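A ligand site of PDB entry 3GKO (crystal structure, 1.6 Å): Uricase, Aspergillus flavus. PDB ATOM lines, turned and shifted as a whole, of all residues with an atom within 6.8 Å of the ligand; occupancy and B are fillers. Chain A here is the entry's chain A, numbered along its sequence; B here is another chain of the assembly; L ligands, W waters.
An oxygen (O1) of the ligand lies within hydrogen-bond range of the backbone NH of Val 227 (3.0 Å).
An oxygen (O1) of the ligand is in hydrogen-bond range of the guanidinium group (NH2) of Arg 176 (2.8 Å).
The side-chain amide nitrogen (NE2) of Gln 228 sits at hydrogen-bond distance from an oxygen (O2) of the ligand, 2.9 Å away.
The backbone NH (N) of Thr 57 of chain B sits at hydrogen-bond distance from a nitrogen (N3) of the ligand (2.8 Å).
ND2 of Asn 254 sits close to N2 of the ligand (3.5 Å).
The side-chain hydroxyl (OG1) of Thr 57 of chain B sits at hydrogen-bond distance from a nitrogen (N3) of the ligand (3.3 Å).
N of Arg 176 sits at hydrogen-bond distance from O of Ser 157, 2.9 Å away.
The backbone NH (N) of Asn 254 sits at hydrogen-bond distance from the backbone carbonyl oxygen (O) of Gly 286, 2.7 Å away.
O of Asn 254 lies within hydrogen-bond range of NE2 of His 256 (3.4 Å).
The backbone carbonyl oxygen of Val 55 of chain B sits at hydrogen-bond distance from the side-chain hydroxyl of Tyr 8 of chain B (2.6 Å).
OG1 of Thr 57 of chain B sits at hydrogen-bond distance from NZ of Lys 10 of chain B, 2.9 Å away.
O of Ser 226 sits at hydrogen-bond distance from OG of Ser 224 (2.8 Å).
The backbone NH of Gln 228 sits close to the side-chain hydroxyl of Ser 226 (3.4 Å).
Residues that only touch the ligand: Phe 159 (3.3 Å), Leu 170 (3.6 Å), Ser 226 (3.6 Å), Tyr 8 of chain B (3.8 Å), Ile 54 of chain B (3.5 Å), Ala 56 of chain B (3.5 Å) and Asp 58 of chain B (3.8 Å).
Hydrophobic or aromatic side chains that line the ligand: Phe 159, Leu 170, Val 227, Tyr 8 of chain B, Ile 54 of chain B and Ala 56 of chain B.
Of the 26 residues printed, 12 come within 4 Å of the ligand.
The nearest printed residue that does not touch the ligand is Ile 288 (4.1 Å).
Water W1 lies within hydrogen-bond range of a nitrogen (N5) of the ligand (2.9 Å) and the guanidinium group (NH1) of Arg 176 (3.3 Å).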
ATOM      1  N   SER A 157      22.236  12.205 -10.998  1.00  0.00           N
ATOM      2  CA  SER A 157      21.898  13.123 -12.077  1.00  0.00           C
ATOM      3  C   SER A 157      21.857  12.186 -13.272  1.00  0.00           C
ATOM      4  O   SER A 157      22.756  11.364 -13.452  1.00  0.00           O
ATOM      5  CB  SER A 157      22.968  14.182 -12.306  1.00  0.00           C
ATOM      6  OG  SER A 157      22.643  14.954 -13.451  1.00  0.00           O
ATOM      7  N   GLN A 158      20.803  12.293 -14.068  1.00  0.00           N
ATOM      8  CA  GLN A 158      20.629  11.433 -15.225  1.00  0.00           C
ATOM      9  C   GLN A 158      20.157  12.248 -16.422  1.00  0.00           C
ATOM     10  O   GLN A 158      19.695  13.368 -16.274  1.00  0.00           O
ATOM     11  CB  GLN A 158      19.571  10.361 -14.928  1.00  0.00           C
ATOM     12  CG  GLN A 158      19.786   9.557 -13.662  1.00  0.00           C
ATOM     13  CD  GLN A 158      18.662   8.561 -13.421  1.00  0.00           C
ATOM     14  OE1 GLN A 158      18.220   7.890 -14.347  1.00  0.00           O
ATOM     15  NE2 GLN A 158      18.217   8.455 -12.174  1.00  0.00           N
ATOM     16  N   PHE A 159      20.297  11.662 -17.596  1.00  0.00           N
ATOM     17  CA  PHE A 159      19.795  12.292 -18.799  1.00  0.00           C
ATOM     18  C   PHE A 159      19.659  11.280 -19.923  1.00  0.00           C
ATOM     19  O   PHE A 159      20.627  10.942 -20.614  1.00  0.00           O
ATOM     20  CB  PHE A 159      20.662  13.465 -19.263  1.00  0.00           C
ATOM     21  CG  PHE A 159      19.976  14.328 -20.290  1.00  0.00           C
ATOM     22  CD1 PHE A 159      18.783  14.967 -19.984  1.00  0.00           C
ATOM     23  CD2 PHE A 159      20.476  14.426 -21.592  1.00  0.00           C
ATOM     24  CE1 PHE A 159      18.077  15.688 -20.946  1.00  0.00           C
ATOM     25  CE2 PHE A 159      19.783  15.149 -22.561  1.00  0.00           C
ATOM     26  CZ  PHE A 159      18.584  15.780 -22.238  1.00  0.00           C
ATOM     27  N   PHE A 162      15.999  11.572 -24.490  1.00  0.00           N
ATOM     28  CA  PHE A 162      15.937  12.767 -25.318  1.00  0.00           C
ATOM     29  C   PHE A 162      15.840  12.411 -26.800  1.00  0.00           C
ATOM     30  O   PHE A 162      16.121  11.274 -27.191  1.00  0.00           O
ATOM     31  CB  PHE A 162      17.160  13.664 -25.074  1.00  0.00           C
ATOM     32  CG  PHE A 162      18.467  12.948 -25.100  1.00  0.00           C
ATOM     33  CD1 PHE A 162      18.964  12.315 -23.958  1.00  0.00           C
ATOM     34  CD2 PHE A 162      19.222  12.892 -26.273  1.00  0.00           C
ATOM     35  CE1 PHE A 162      20.184  11.654 -23.974  1.00  0.00           C
ATOM     36  CE2 PHE A 162      20.454  12.234 -26.296  1.00  0.00           C
ATOM     37  CZ  PHE A 162      20.929  11.610 -25.146  1.00  0.00           C
ATOM     38  N   LEU A 170      25.252  12.252 -28.480  1.00  0.00           N
ATOM     39  CA  LEU A 170      25.231  12.117 -27.032  1.00  0.00           C
ATOM     40  C   LEU A 170      24.661  10.784 -26.567  1.00  0.00           C
ATOM     41  O   LEU A 170      23.566  10.394 -26.965  1.00  0.00           O
ATOM     42  CB  LEU A 170      24.415  13.255 -26.393  1.00  0.00           C
ATOM     43  CG  LEU A 170      24.303  13.261 -24.861  1.00  0.00           C
ATOM     44  CD1 LEU A 170      25.673  13.516 -24.237  1.00  0.00           C
ATOM     45  CD2 LEU A 170      23.322  14.343 -24.433  1.00  0.00           C
ATOM     46  N   ARG A 176      25.506  10.650 -13.994  1.00  0.00           N
ATOM     47  CA  ARG A 176      26.467  11.640 -14.457  1.00  0.00           C
ATOM     48  C   ARG A 176      26.680  12.703 -13.397  1.00  0.00           C
ATOM     49  O   ARG A 176      25.980  12.760 -12.390  1.00  0.00           O
ATOM     50  CB  ARG A 176      25.972  12.310 -15.743  1.00  0.00           C
ATOM     51  CG  ARG A 176      24.740  13.188 -15.533  1.00  0.00           C
ATOM     52  CD  ARG A 176      24.290  13.937 -16.777  1.00  0.00           C
ATOM     53  NE  ARG A 176      23.213  14.878 -16.438  1.00  0.00           N
ATOM     54  CZ  ARG A 176      22.671  15.746 -17.285  1.00  0.00           C
ATOM     55  NH1 ARG A 176      23.080  15.814 -18.541  1.00  0.00           N
ATOM     56  NH2 ARG A 176      21.717  16.570 -16.855  1.00  0.00           N
ATOM     57  N   LEU A 178      26.637  16.634 -12.221  1.00  0.00           N
ATOM     58  CA  LEU A 178      25.839  17.821 -12.516  1.00  0.00           C
ATOM     59  C   LEU A 178      26.416  18.970 -11.709  1.00  0.00           C
ATOM     60  O   LEU A 178      26.499  18.920 -10.486  1.00  0.00           O
ATOM     61  CB  LEU A 178      24.359  17.610 -12.159  1.00  0.00           C
ATOM     62  CG  LEU A 178      23.475  18.847 -12.366  1.00  0.00           C
ATOM     63  CD1 LEU A 178      23.528  19.294 -13.815  1.00  0.00           C
ATOM     64  CD2 LEU A 178      22.044  18.509 -11.960  1.00  0.00           C
ATOM     65  N   SER A 224      17.904  13.907 -10.278  1.00  0.00           N
ATOM     66  CA  SER A 224      17.605  14.675 -11.485  1.00  0.00           C
ATOM     67  C   SER A 224      17.437  13.948 -12.820  1.00  0.00           C
ATOM     68  O   SER A 224      18.319  13.204 -13.248  1.00  0.00           O
ATOM     69  CB  SER A 224      18.669  15.762 -11.634  1.00  0.00           C
ATOM     70  OG  SER A 224      18.399  16.578 -12.761  1.00  0.00           O
ATOM     71  N   ALA A 225      16.308  14.206 -13.465  1.00  0.00           N
ATOM     72  CA  ALA A 225      15.999  13.624 -14.766  1.00  0.00           C
ATOM     73  C   ALA A 225      16.572  14.528 -15.854  1.00  0.00           C
ATOM     74  O   ALA A 225      16.755  14.125 -16.995  1.00  0.00           O
ATOM     75  CB  ALA A 225      14.491  13.488 -14.940  1.00  0.00           C
ATOM     76  N   SER A 226      16.844  15.775 -15.464  1.00  0.00           N
ATOM     77  CA  SER A 226      17.396  16.785 -16.358  1.00  0.00           C
ATOM     78  C   SER A 226      17.501  18.087 -15.569  1.00  0.00           C
ATOM     79  O   SER A 226      16.899  18.209 -14.498  1.00  0.00           O
ATOM     80  CB  SER A 226      16.481  17.013 -17.570  1.00  0.00           C
ATOM     81  OG  SER A 226      15.268  17.627 -17.167  1.00  0.00           O
ATOM     82  N   VAL A 227      18.231  19.058 -16.085  1.00  0.00           N
ATOM     83  CA  VAL A 227      18.350  20.337 -15.407  1.00  0.00           C
ATOM     84  C   VAL A 227      16.948  20.956 -15.402  1.00  0.00           C
ATOM     85  O   VAL A 227      16.513  21.517 -14.399  1.00  0.00           O
ATOM     86  CB  VAL A 227      19.337  21.275 -16.128  1.00  0.00           C
ATOM     87  CG1 VAL A 227      19.302  22.667 -15.507  1.00  0.00           C
ATOM     88  CG2 VAL A 227      20.744  20.709 -16.036  1.00  0.00           C
ATOM     89  N   GLN A 228      16.252  20.828 -16.525  1.00  0.00           N
ATOM     90  CA  GLN A 228      14.898  21.350 -16.690  1.00  0.00           C
ATOM     91  C   GLN A 228      13.943  20.860 -15.592  1.00  0.00           C
ATOM     92  O   GLN A 228      13.260  21.672 -14.959  1.00  0.00           O
ATOM     93  CB  GLN A 228      14.331  20.936 -18.057  1.00  0.00           C
ATOM     94  CG  GLN A 228      14.971  21.644 -19.251  1.00  0.00           C
ATOM     95  CD  GLN A 228      16.178  20.915 -19.828  1.00  0.00           C
ATOM     96  OE1 GLN A 228      16.939  20.269 -19.112  1.00  0.00           O
ATOM     97  NE2 GLN A 228      16.361  21.026 -21.151  1.00  0.00           N
ATOM     98  N   ASN A 254      24.855  24.199 -17.658  1.00  0.00           N
ATOM     99  CA  ASN A 254      25.186  22.823 -17.347  1.00  0.00           C
ATOM    100  C   ASN A 254      26.688  22.794 -17.626  1.00  0.00           C
ATOM    101  O   ASN A 254      27.110  22.731 -18.777  1.00  0.00           O
ATOM    102  CB  ASN A 254      24.436  21.854 -18.254  1.00  0.00           C
ATOM    103  CG  ASN A 254      24.507  20.407 -17.752  1.00  0.00           C
ATOM    104  OD1 ASN A 254      25.201  20.102 -16.791  1.00  0.00           O
ATOM    105  ND2 ASN A 254      23.784  19.513 -18.428  1.00  0.00           N
ATOM    106  N   HIS A 256      29.612  20.999 -17.943  1.00  0.00           N
ATOM    107  CA  HIS A 256      29.973  19.621 -18.237  1.00  0.00           C
ATOM    108  C   HIS A 256      31.299  19.086 -17.728  1.00  0.00           C
ATOM    109  O   HIS A 256      32.316  19.772 -17.760  1.00  0.00           O
ATOM    110  CB  HIS A 256      29.931  19.405 -19.759  1.00  0.00           C
ATOM    111  CG  HIS A 256      28.681  19.911 -20.419  1.00  0.00           C
ATOM    112  ND1 HIS A 256      27.431  19.444 -20.107  1.00  0.00           N
ATOM    113  CD2 HIS A 256      28.504  20.859 -21.370  1.00  0.00           C
ATOM    114  CE1 HIS A 256      26.526  20.073 -20.844  1.00  0.00           C
ATOM    115  NE2 HIS A 256      27.157  20.932 -21.621  1.00  0.00           N
ATOM    116  N   GLY A 286      25.746  23.889 -21.600  1.00  0.00           N
ATOM    117  CA  GLY A 286      24.330  23.987 -21.850  1.00  0.00           C
ATOM    118  C   GLY A 286      23.826  25.160 -21.018  1.00  0.00           C
ATOM    119  O   GLY A 286      24.422  25.515 -20.006  1.00  0.00           O
ATOM    120  N   ILE A 288      20.125  26.411 -19.556  1.00  0.00           N
ATOM    121  CA  ILE A 288      18.724  26.076 -19.383  1.00  0.00           C
ATOM    122  C   ILE A 288      17.993  27.171 -18.619  1.00  0.00           C
ATOM    123  O   ILE A 288      18.428  27.561 -17.529  1.00  0.00           O
ATOM    124  CB  ILE A 288      18.586  24.738 -18.610  1.00  0.00           C
ATOM    125  CG1 ILE A 288      19.654  23.746 -19.070  1.00  0.00           C
ATOM    126  CG2 ILE A 288      17.196  24.151 -18.809  1.00  0.00           C
ATOM    127  CD1 ILE A 288      19.585  23.352 -20.524  1.00  0.00           C
ATOM    128  N   TYR B   8      16.148  26.896 -23.942  1.00  0.00           N
ATOM    129  CA  TYR B   8      17.345  26.185 -23.538  1.00  0.00           C
ATOM    130  C   TYR B   8      18.189  25.897 -24.769  1.00  0.00           C
ATOM    131  O   TYR B   8      17.703  25.943 -25.900  1.00  0.00           O
ATOM    132  CB  TYR B   8      16.953  24.856 -22.871  1.00  0.00           C
ATOM    133  CG  TYR B   8      16.636  23.792 -23.896  1.00  0.00           C
ATOM    134  CD1 TYR B   8      15.484  23.887 -24.684  1.00  0.00           C
ATOM    135  CD2 TYR B   8      17.555  22.791 -24.190  1.00  0.00           C
ATOM    136  CE1 TYR B   8      15.275  23.019 -25.752  1.00  0.00           C
ATOM    137  CE2 TYR B   8      17.353  21.916 -25.248  1.00  0.00           C
ATOM    138  CZ  TYR B   8      16.215  22.041 -26.029  1.00  0.00           C
ATOM    139  OH  TYR B   8      16.050  21.215 -27.120  1.00  0.00           O
ATOM    140  N   GLY B   9      19.462  25.597 -24.549  1.00  0.00           N
ATOM    141  CA  GLY B   9      20.342  25.311 -25.674  1.00  0.00           C
ATOM    142  C   GLY B   9      21.794  25.250 -25.254  1.00  0.00           C
ATOM    143  O   GLY B   9      22.106  24.957 -24.105  1.00  0.00           O
ATOM    144  N   LYS B  10      22.693  25.530 -26.194  1.00  0.00           N
ATOM    145  CA  LYS B  10      24.116  25.503 -25.884  1.00  0.00           C
ATOM    146  C   LYS B  10      24.703  26.907 -26.043  1.00  0.00           C
ATOM    147  O   LYS B  10      24.447  27.578 -27.038  1.00  0.00           O
ATOM    148  CB  LYS B  10      24.853  24.526 -26.798  1.00  0.00           C
ATOM    149  CG  LYS B  10      26.271  24.180 -26.317  1.00  0.00           C
ATOM    150  CD  LYS B  10      26.260  23.274 -25.096  1.00  0.00           C
ATOM    151  CE  LYS B  10      26.287  21.805 -25.491  1.00  0.00           C
ATOM    152  NZ  LYS B  10      26.138  20.900 -24.305  1.00  0.00           N
ATOM    153  N   ASN B  51      11.814  14.072 -21.538  1.00  0.00           N
ATOM    154  CA  ASN B  51      12.929  14.482 -22.376  1.00  0.00           C
ATOM    155  C   ASN B  51      12.726  14.234 -23.864  1.00  0.00           C
ATOM    156  O   ASN B  51      13.560  14.633 -24.677  1.00  0.00           O
ATOM    157  CB  ASN B  51      14.219  13.809 -21.900  1.00  0.00           C
ATOM    158  CG  ASN B  51      14.661  14.303 -20.525  1.00  0.00           C
ATOM    159  OD1 ASN B  51      14.435  15.467 -20.171  1.00  0.00           O
ATOM    160  ND2 ASN B  51      15.298  13.438 -19.760  1.00  0.00           N
ATOM    161  N   ILE B  54      13.115  17.191 -25.945  1.00  0.00           N
ATOM    162  CA  ILE B  54      14.396  17.867 -25.915  1.00  0.00           C
ATOM    163  C   ILE B  54      15.389  17.484 -27.013  1.00  0.00           C
ATOM    164  O   ILE B  54      15.765  16.315 -27.144  1.00  0.00           O
ATOM    165  CB  ILE B  54      15.129  17.645 -24.564  1.00  0.00           C
ATOM    166  CG1 ILE B  54      14.315  18.228 -23.413  1.00  0.00           C
ATOM    167  CG2 ILE B  54      16.521  18.299 -24.611  1.00  0.00           C
ATOM    168  CD1 ILE B  54      14.954  18.027 -22.049  1.00  0.00           C
ATOM    169  N   VAL B  55      15.764  18.473 -27.803  1.00  0.00           N
ATOM    170  CA  VAL B  55      16.780  18.294 -28.819  1.00  0.00           C
ATOM    171  C   VAL B  55      17.990  18.577 -27.922  1.00  0.00           C
ATOM    172  O   VAL B  55      18.182  19.719 -27.494  1.00  0.00           O
ATOM    173  CB  VAL B  55      16.677  19.372 -29.926  1.00  0.00           C
ATOM    174  CG1 VAL B  55      17.886  19.278 -30.859  1.00  0.00           C
ATOM    175  CG2 VAL B  55      15.394  19.177 -30.725  1.00  0.00           C
ATOM    176  N   ALA B  56      18.780  17.551 -27.611  1.00  0.00           N
ATOM    177  CA  ALA B  56      19.926  17.704 -26.717  1.00  0.00           C
ATOM    178  C   ALA B  56      20.796  18.903 -27.052  1.00  0.00           C
ATOM    179  O   ALA B  56      21.062  19.180 -28.221  1.00  0.00           O
ATOM    180  CB  ALA B  56      20.776  16.421 -26.729  1.00  0.00           C
ATOM    181  N   THR B  57      21.240  19.623 -26.020  1.00  0.00           N
ATOM    182  CA  THR B  57      22.083  20.785 -26.278  1.00  0.00           C
ATOM    183  C   THR B  57      23.359  20.313 -26.951  1.00  0.00           C
ATOM    184  O   THR B  57      23.966  21.063 -27.707  1.00  0.00           O
ATOM    185  CB  THR B  57      22.434  21.536 -24.985  1.00  0.00           C
ATOM    186  OG1 THR B  57      23.277  20.726 -24.169  1.00  0.00           O
ATOM    187  CG2 THR B  57      21.162  21.911 -24.229  1.00  0.00           C
ATOM    188  N   ASP B  58      23.765  19.075 -26.675  1.00  0.00           N
ATOM    189  CA  ASP B  58      24.965  18.530 -27.306  1.00  0.00           C
ATOM    190  C   ASP B  58      24.701  18.410 -28.799  1.00  0.00           C
ATOM    191  O   ASP B  58      25.600  18.630 -29.617  1.00  0.00           O
ATOM    192  CB  ASP B  58      25.295  17.138 -26.758  1.00  0.00           C
ATOM    193  CG  ASP B  58      26.609  16.599 -27.300  1.00  0.00           C
ATOM    194  OD1 ASP B  58      27.680  17.038 -26.817  1.00  0.00           O
ATOM    195  OD2 ASP B  58      26.568  15.764 -28.226  1.00  0.00           O
ATOM    196  N   SER B  59      23.469  18.065 -29.165  1.00  0.00           N
ATOM    197  CA  SER B  59      23.089  17.942 -30.572  1.00  0.00           C
ATOM    198  C   SER B  59      23.040  19.328 -31.200  1.00  0.00           C
ATOM    199  O   SER B  59      23.373  19.502 -32.372  1.00  0.00           O
ATOM    200  CB  SER B  59      21.727  17.254 -30.706  1.00  0.00           C
ATOM    201  OG  SER B  59      21.758  15.962 -30.108  1.00  0.00           O
HETATM  202  N1  LIG L   1      19.328  19.011 -20.282  1.00  0.00           N
HETATM  203  C1  LIG L   1      20.200  18.310 -19.509  1.00  0.00           C
HETATM  204  O1  LIG L   1      20.004  18.238 -18.310  1.00  0.00           O
HETATM  205  N2  LIG L   1      21.287  17.678 -20.045  1.00  0.00           N
HETATM  206  C2  LIG L   1      21.546  17.731 -21.416  1.00  0.00           C
HETATM  207  C3  LIG L   1      20.671  18.443 -22.255  1.00  0.00           C
HETATM  208  C4  LIG L   1      19.497  19.116 -21.637  1.00  0.00           C
HETATM  209  O2  LIG L   1      18.714  19.755 -22.316  1.00  0.00           O
HETATM  210  N3  LIG L   1      21.127  18.353 -23.512  1.00  0.00           N
HETATM  211  N4  LIG L   1      22.210  17.647 -23.516  1.00  0.00           N
HETATM  212  N5  LIG L   1      22.513  17.231 -22.208  1.00  0.00           N
HETATM  213  O   HOH W   1      25.010  16.237 -21.149  1.00  0.00           O
